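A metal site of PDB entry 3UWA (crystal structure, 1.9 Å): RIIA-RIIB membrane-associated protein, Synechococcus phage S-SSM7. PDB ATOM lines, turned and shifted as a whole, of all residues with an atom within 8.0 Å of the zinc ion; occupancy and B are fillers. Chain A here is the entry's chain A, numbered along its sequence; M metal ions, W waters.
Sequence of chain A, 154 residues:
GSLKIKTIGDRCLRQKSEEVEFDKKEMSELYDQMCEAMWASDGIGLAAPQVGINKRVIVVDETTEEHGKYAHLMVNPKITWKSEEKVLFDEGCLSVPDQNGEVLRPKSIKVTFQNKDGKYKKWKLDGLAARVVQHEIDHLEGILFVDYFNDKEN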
ATOM      1  N   LEU A  13     -35.169   1.729  22.352  1.00  0.00           N
ATOM      2  CA  LEU A  13     -33.786   2.035  21.949  1.00  0.00           C
ATOM      3  C   LEU A  13     -33.132   3.107  22.835  1.00  0.00           C
ATOM      4  O   LEU A  13     -31.933   3.325  22.761  1.00  0.00           O
ATOM      5  CB  LEU A  13     -33.764   2.511  20.493  1.00  0.00           C
ATOM      6  CG  LEU A  13     -34.085   1.434  19.463  1.00  0.00           C
ATOM      7  CD1 LEU A  13     -34.194   2.040  18.071  1.00  0.00           C
ATOM      8  CD2 LEU A  13     -33.016   0.354  19.532  1.00  0.00           C
ATOM      9  N   GLY A  45     -22.143  -5.761  13.874  1.00  0.00           N
ATOM     10  CA  GLY A  45     -22.424  -5.689  15.310  1.00  0.00           C
ATOM     11  C   GLY A  45     -23.902  -5.605  15.573  1.00  0.00           C
ATOM     12  O   GLY A  45     -24.687  -5.231  14.683  1.00  0.00           O
ATOM     13  N   LEU A  46     -24.285  -5.964  16.802  1.00  0.00           N
ATOM     14  CA  LEU A  46     -25.663  -5.843  17.239  1.00  0.00           C
ATOM     15  C   LEU A  46     -25.742  -5.842  18.763  1.00  0.00           C
ATOM     16  O   LEU A  46     -25.017  -6.557  19.453  1.00  0.00           O
ATOM     17  CB  LEU A  46     -26.527  -7.002  16.691  1.00  0.00           C
ATOM     18  CG  LEU A  46     -28.039  -6.743  16.583  1.00  0.00           C
ATOM     19  CD1 LEU A  46     -28.381  -5.791  15.404  1.00  0.00           C
ATOM     20  CD2 LEU A  46     -28.875  -8.011  16.500  1.00  0.00           C
ATOM     21  N   ALA A  47     -26.680  -5.060  19.300  1.00  0.00           N
ATOM     22  CA  ALA A  47     -26.894  -4.992  20.740  1.00  0.00           C
ATOM     23  C   ALA A  47     -28.291  -5.522  21.026  1.00  0.00           C
ATOM     24  O   ALA A  47     -29.202  -5.345  20.235  1.00  0.00           O
ATOM     25  CB  ALA A  47     -26.705  -3.543  21.223  1.00  0.00           C
ATOM     26  N   GLN A  50     -31.605  -3.501  20.402  1.00  0.00           N
ATOM     27  CA  GLN A  50     -32.030  -3.434  18.990  1.00  0.00           C
ATOM     28  C   GLN A  50     -33.017  -4.511  18.608  1.00  0.00           C
ATOM     29  O   GLN A  50     -33.730  -4.331  17.666  1.00  0.00           O
ATOM     30  CB  GLN A  50     -30.856  -3.541  18.030  1.00  0.00           C
ATOM     31  CG  GLN A  50     -29.837  -2.462  18.203  1.00  0.00           C
ATOM     32  CD  GLN A  50     -28.763  -2.545  17.179  1.00  0.00           C
ATOM     33  OE1 GLN A  50     -27.678  -3.065  17.475  1.00  0.00           O
ATOM     34  NE2 GLN A  50     -29.054  -2.103  15.962  1.00  0.00           N
ATOM     35  N   GLU A  91     -20.168   5.809  10.214  1.00  0.00           N
ATOM     36  CA  GLU A  91     -21.032   4.823  10.847  1.00  0.00           C
ATOM     37  C   GLU A  91     -22.409   4.683  10.215  1.00  0.00           C
ATOM     38  O   GLU A  91     -22.935   5.605   9.619  1.00  0.00           O
ATOM     39  CB  GLU A  91     -21.212   5.167  12.338  1.00  0.00           C
ATOM     40  CG  GLU A  91     -19.892   5.035  13.083  1.00  0.00           C
ATOM     41  CD  GLU A  91     -20.005   5.070  14.589  1.00  0.00           C
ATOM     42  OE1 GLU A  91     -21.095   4.744  15.150  1.00  0.00           O
ATOM     43  OE2 GLU A  91     -18.955   5.398  15.217  1.00  0.00           O
ATOM     44  N   GLY A  92     -22.983   3.497  10.372  1.00  0.00           N
ATOM     45  CA  GLY A  92     -24.382   3.269  10.159  1.00  0.00           C
ATOM     46  C   GLY A  92     -24.856   2.369  11.257  1.00  0.00           C
ATOM     47  O   GLY A  92     -24.099   2.022  12.169  1.00  0.00           O
ATOM     48  N   CYS A  93     -26.130   1.957  11.159  1.00  0.00           N
ATOM     49  CA  CYS A  93     -26.773   1.180  12.218  1.00  0.00           C
ATOM     50  C   CYS A  93     -28.064   0.583  11.659  1.00  0.00           C
ATOM     51  O   CYS A  93     -28.851   1.279  10.988  1.00  0.00           O
ATOM     52  CB  CYS A  93     -27.096   2.090  13.416  1.00  0.00           C
ATOM     53  SG  CYS A  93     -27.856   1.230  14.805  1.00  0.00           S
ATOM     54  N   LEU A  94     -28.268  -0.699  11.923  1.00  0.00           N
ATOM     55  CA  LEU A  94     -29.486  -1.375  11.488  1.00  0.00           C
ATOM     56  C   LEU A  94     -30.725  -0.770  12.125  1.00  0.00           C
ATOM     57  O   LEU A  94     -31.820  -0.844  11.535  1.00  0.00           O
ATOM     58  CB  LEU A  94     -29.400  -2.879  11.757  1.00  0.00           C
ATOM     59  CG  LEU A  94     -28.365  -3.624  10.884  1.00  0.00           C
ATOM     60  CD1 LEU A  94     -28.272  -5.105  11.245  1.00  0.00           C
ATOM     61  CD2 LEU A  94     -28.718  -3.419   9.398  1.00  0.00           C
ATOM     62  N   SER A  95     -30.560  -0.159  13.310  1.00  0.00           N
ATOM     63  CA  SER A  95     -31.682   0.552  13.955  1.00  0.00           C
ATOM     64  C   SER A  95     -31.915   2.004  13.477  1.00  0.00           C
ATOM     65  O   SER A  95     -32.870   2.656  13.950  1.00  0.00           O
ATOM     66  CB  SER A  95     -31.523   0.501  15.462  1.00  0.00           C
ATOM     67  OG  SER A  95     -31.677  -0.816  15.920  1.00  0.00           O
ATOM     68  N   VAL A  96     -31.067   2.486  12.565  1.00  0.00           N
ATOM     69  CA  VAL A  96     -31.144   3.834  12.004  1.00  0.00           C
ATOM     70  C   VAL A  96     -30.976   3.719  10.471  1.00  0.00           C
ATOM     71  O   VAL A  96     -30.010   4.162   9.875  1.00  0.00           O
ATOM     72  CB  VAL A  96     -30.086   4.791  12.606  1.00  0.00           C
ATOM     73  CG1 VAL A  96     -30.413   6.221  12.236  1.00  0.00           C
ATOM     74  CG2 VAL A  96     -29.971   4.647  14.130  1.00  0.00           C
ATOM     75  N   ARG A 105     -14.420   8.861  17.670  1.00  0.00           N
ATOM     76  CA  ARG A 105     -14.354   8.122  18.937  1.00  0.00           C
ATOM     77  C   ARG A 105     -12.939   7.754  19.204  1.00  0.00           C
ATOM     78  O   ARG A 105     -12.128   7.760  18.277  1.00  0.00           O
ATOM     79  CB  ARG A 105     -15.155   6.809  18.900  1.00  0.00           C
ATOM     80  CG  ARG A 105     -16.562   6.892  18.335  1.00  0.00           C
ATOM     81  CD  ARG A 105     -17.199   5.524  18.502  1.00  0.00           C
ATOM     82  NE  ARG A 105     -18.535   5.426  17.951  1.00  0.00           N
ATOM     83  CZ  ARG A 105     -19.668   5.422  18.648  1.00  0.00           C
ATOM     84  NH1 ARG A 105     -19.712   5.579  19.976  1.00  0.00           N
ATOM     85  NH2 ARG A 105     -20.810   5.266  17.986  1.00  0.00           N
ATOM     86  N   VAL A 132     -16.676  -0.882  16.631  1.00  0.00           N
ATOM     87  CA  VAL A 132     -17.950  -1.630  16.723  1.00  0.00           C
ATOM     88  C   VAL A 132     -18.333  -1.816  18.171  1.00  0.00           C
ATOM     89  O   VAL A 132     -19.482  -1.582  18.523  1.00  0.00           O
ATOM     90  CB  VAL A 132     -17.876  -2.976  15.998  1.00  0.00           C
ATOM     91  CG1 VAL A 132     -19.186  -3.776  16.192  1.00  0.00           C
ATOM     92  CG2 VAL A 132     -17.501  -2.792  14.546  1.00  0.00           C
ATOM     93  N   HIS A 135     -19.688   1.571  19.606  1.00  0.00           N
ATOM     94  CA  HIS A 135     -21.024   1.779  19.019  1.00  0.00           C
ATOM     95  C   HIS A 135     -22.070   0.894  19.672  1.00  0.00           C
ATOM     96  O   HIS A 135     -23.172   1.353  20.052  1.00  0.00           O
ATOM     97  CB  HIS A 135     -20.984   1.510  17.497  1.00  0.00           C
ATOM     98  CG  HIS A 135     -22.320   1.624  16.796  1.00  0.00           C
ATOM     99  ND1 HIS A 135     -22.614   2.631  15.912  1.00  0.00           N
ATOM    100  CD2 HIS A 135     -23.430   0.792  16.827  1.00  0.00           C
ATOM    101  CE1 HIS A 135     -23.860   2.472  15.442  1.00  0.00           C
ATOM    102  NE2 HIS A 135     -24.377   1.344  15.993  1.00  0.00           N
ATOM    103  N   GLU A 136     -21.744  -0.396  19.808  1.00  0.00           N
ATOM    104  CA  GLU A 136     -22.704  -1.346  20.411  1.00  0.00           C
ATOM    105  C   GLU A 136     -22.952  -1.120  21.913  1.00  0.00           C
ATOM    106  O   GLU A 136     -24.116  -1.240  22.380  1.00  0.00           O
ATOM    107  CB  GLU A 136     -22.306  -2.802  20.151  1.00  0.00           C
ATOM    108  CG  GLU A 136     -22.252  -3.203  18.644  1.00  0.00           C
ATOM    109  CD  GLU A 136     -23.549  -2.887  17.901  1.00  0.00           C
ATOM    110  OE1 GLU A 136     -24.631  -2.913  18.527  1.00  0.00           O
ATOM    111  OE2 GLU A 136     -23.494  -2.584  16.673  1.00  0.00           O
ATOM    112  N   ILE A 137     -21.913  -0.839  22.680  1.00  0.00           N
ATOM    113  CA  ILE A 137     -22.092  -0.508  24.104  1.00  0.00           C
ATOM    114  C   ILE A 137     -22.934   0.767  24.243  1.00  0.00           C
ATOM    115  O   ILE A 137     -23.742   0.854  25.164  1.00  0.00           O
ATOM    116  CB  ILE A 137     -20.754  -0.395  24.878  1.00  0.00           C
ATOM    117  CG1 ILE A 137     -20.062  -1.775  24.984  1.00  0.00           C
ATOM    118  CG2 ILE A 137     -20.981   0.233  26.253  1.00  0.00           C
ATOM    119  CD1 ILE A 137     -18.680  -1.772  25.651  1.00  0.00           C
ATOM    120  N   ASP A 138     -22.789   1.737  23.319  1.00  0.00           N
ATOM    121  CA  ASP A 138     -23.653   2.952  23.321  1.00  0.00           C
ATOM    122  C   ASP A 138     -25.140   2.560  23.324  1.00  0.00           C
ATOM    123  O   ASP A 138     -25.924   3.182  24.068  1.00  0.00           O
ATOM    124  CB  ASP A 138     -23.403   3.903  22.142  1.00  0.00           C
ATOM    125  CG  ASP A 138     -22.308   4.930  22.421  1.00  0.00           C
ATOM    126  OD1 ASP A 138     -21.738   4.908  23.508  1.00  0.00           O
ATOM    127  OD2 ASP A 138     -22.011   5.771  21.552  1.00  0.00           O
ATOM    128  N   HIS A 139     -25.520   1.540  22.528  1.00  0.00           N
ATOM    129  CA  HIS A 139     -26.932   1.043  22.546  1.00  0.00           C
ATOM    130  C   HIS A 139     -27.423   0.678  23.930  1.00  0.00           C
ATOM    131  O   HIS A 139     -28.600   0.875  24.243  1.00  0.00           O
ATOM    132  CB  HIS A 139     -27.159  -0.161  21.620  1.00  0.00           C
ATOM    133  CG  HIS A 139     -27.271   0.184  20.154  1.00  0.00           C
ATOM    134  ND1 HIS A 139     -28.265   0.993  19.664  1.00  0.00           N
ATOM    135  CD2 HIS A 139     -26.499  -0.194  19.077  1.00  0.00           C
ATOM    136  CE1 HIS A 139     -28.113   1.091  18.316  1.00  0.00           C
ATOM    137  NE2 HIS A 139     -27.029   0.383  17.958  1.00  0.00           N
ATOM    138  N   ILE A 143     -28.032   5.185  23.662  1.00  0.00           N
ATOM    139  CA  ILE A 143     -27.403   6.151  22.750  1.00  0.00           C
ATOM    140  C   ILE A 143     -27.387   5.597  21.328  1.00  0.00           C
ATOM    141  O   ILE A 143     -26.971   4.457  21.086  1.00  0.00           O
ATOM    142  CB  ILE A 143     -25.935   6.479  23.172  1.00  0.00           C
ATOM    143  CG1 ILE A 143     -25.876   7.122  24.560  1.00  0.00           C
ATOM    144  CG2 ILE A 143     -25.249   7.404  22.161  1.00  0.00           C
ATOM    145  CD1 ILE A 143     -24.457   7.114  25.155  1.00  0.00           C
ATOM    146  N   LEU A 144     -27.863   6.408  20.379  1.00  0.00           N
ATOM    147  CA  LEU A 144     -27.767   6.101  18.949  1.00  0.00           C
ATOM    148  C   LEU A 144     -26.676   6.987  18.320  1.00  0.00           C
ATOM    149  O   LEU A 144     -26.448   8.081  18.782  1.00  0.00           O
ATOM    150  CB  LEU A 144     -29.123   6.356  18.287  1.00  0.00           C
ATOM    151  CG  LEU A 144     -30.299   5.528  18.827  1.00  0.00           C
ATOM    152  CD1 LEU A 144     -31.557   5.929  18.080  1.00  0.00           C
ATOM    153  CD2 LEU A 144     -29.997   4.040  18.737  1.00  0.00           C
ATOM    154  N   PHE A 145     -26.046   6.526  17.249  1.00  0.00           N
ATOM    155  CA  PHE A 145     -24.858   7.241  16.716  1.00  0.00           C
ATOM    156  C   PHE A 145     -25.162   8.629  16.134  1.00  0.00           C
ATOM    157  O   PHE A 145     -24.291   9.544  16.110  1.00  0.00           O
ATOM    158  CB  PHE A 145     -24.158   6.382  15.678  1.00  0.00           C
ATOM    159  CG  PHE A 145     -24.770   6.439  14.307  1.00  0.00           C
ATOM    160  CD1 PHE A 145     -24.279   7.331  13.364  1.00  0.00           C
ATOM    161  CD2 PHE A 145     -25.795   5.569  13.946  1.00  0.00           C
ATOM    162  CE1 PHE A 145     -24.824   7.385  12.091  1.00  0.00           C
ATOM    163  CE2 PHE A 145     -26.334   5.594  12.650  1.00  0.00           C
ATOM    164  CZ  PHE A 145     -25.849   6.515  11.730  1.00  0.00           C
HETATM  165 ZN    ZN M   1     -26.179   0.283  16.089  1.00  0.00          ZN
HETATM  166  O   HOH W   1     -25.706  -1.664  15.989  1.00  0.00           O
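OE1 of Gln 50 sits at hydrogen-bond distance from N of Ala 47, 2.9 Å away. OE1 of Glu 136 sits close to OE1 of Gln 50 (3.2 Å). N of Ala 47 lies within hydrogen-bond range of OE1 of Glu 136 (3.1 Å). The side-chain sulfur of Cys 93 sits close to the side-chain amide nitrogen of Gln 50 (3.7 Å). A ring nitrogen (ND1) of His 135 is in hydrogen-bond range of the side-chain carboxylate (OE1) of Glu 91, 2.7 Å away. The side-chain amide nitrogen (NE2) of Gln 50 sits at hydrogen-bond distance from the side-chain hydroxyl (OG) of Ser 95 (2.9 Å). The backbone NH (N) of Leu 46 lies close to the side-chain carboxylate (OE2) of Glu 136 (3.5 Å). The side-chain sulfur (SG) of Cys 93 lies close to the backbone NH (N) of Ser 95 (3.4 Å).
The zinc ion is bound by water W1, a ring nitrogen (NE2) of His 139, a ring nitrogen (NE2) of His 135 and the side-chain sulfur of Cys 93.
Residues that only touch the zinc ion: Gln 50 and Glu 136. Five residues have an atom within 4 Å of the zinc ion: Gln 50, Cys 93, His 135, Glu 136 and His 139.
Water W1 bridges OE2 of Glu 136 and OE1 of Gln 50.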
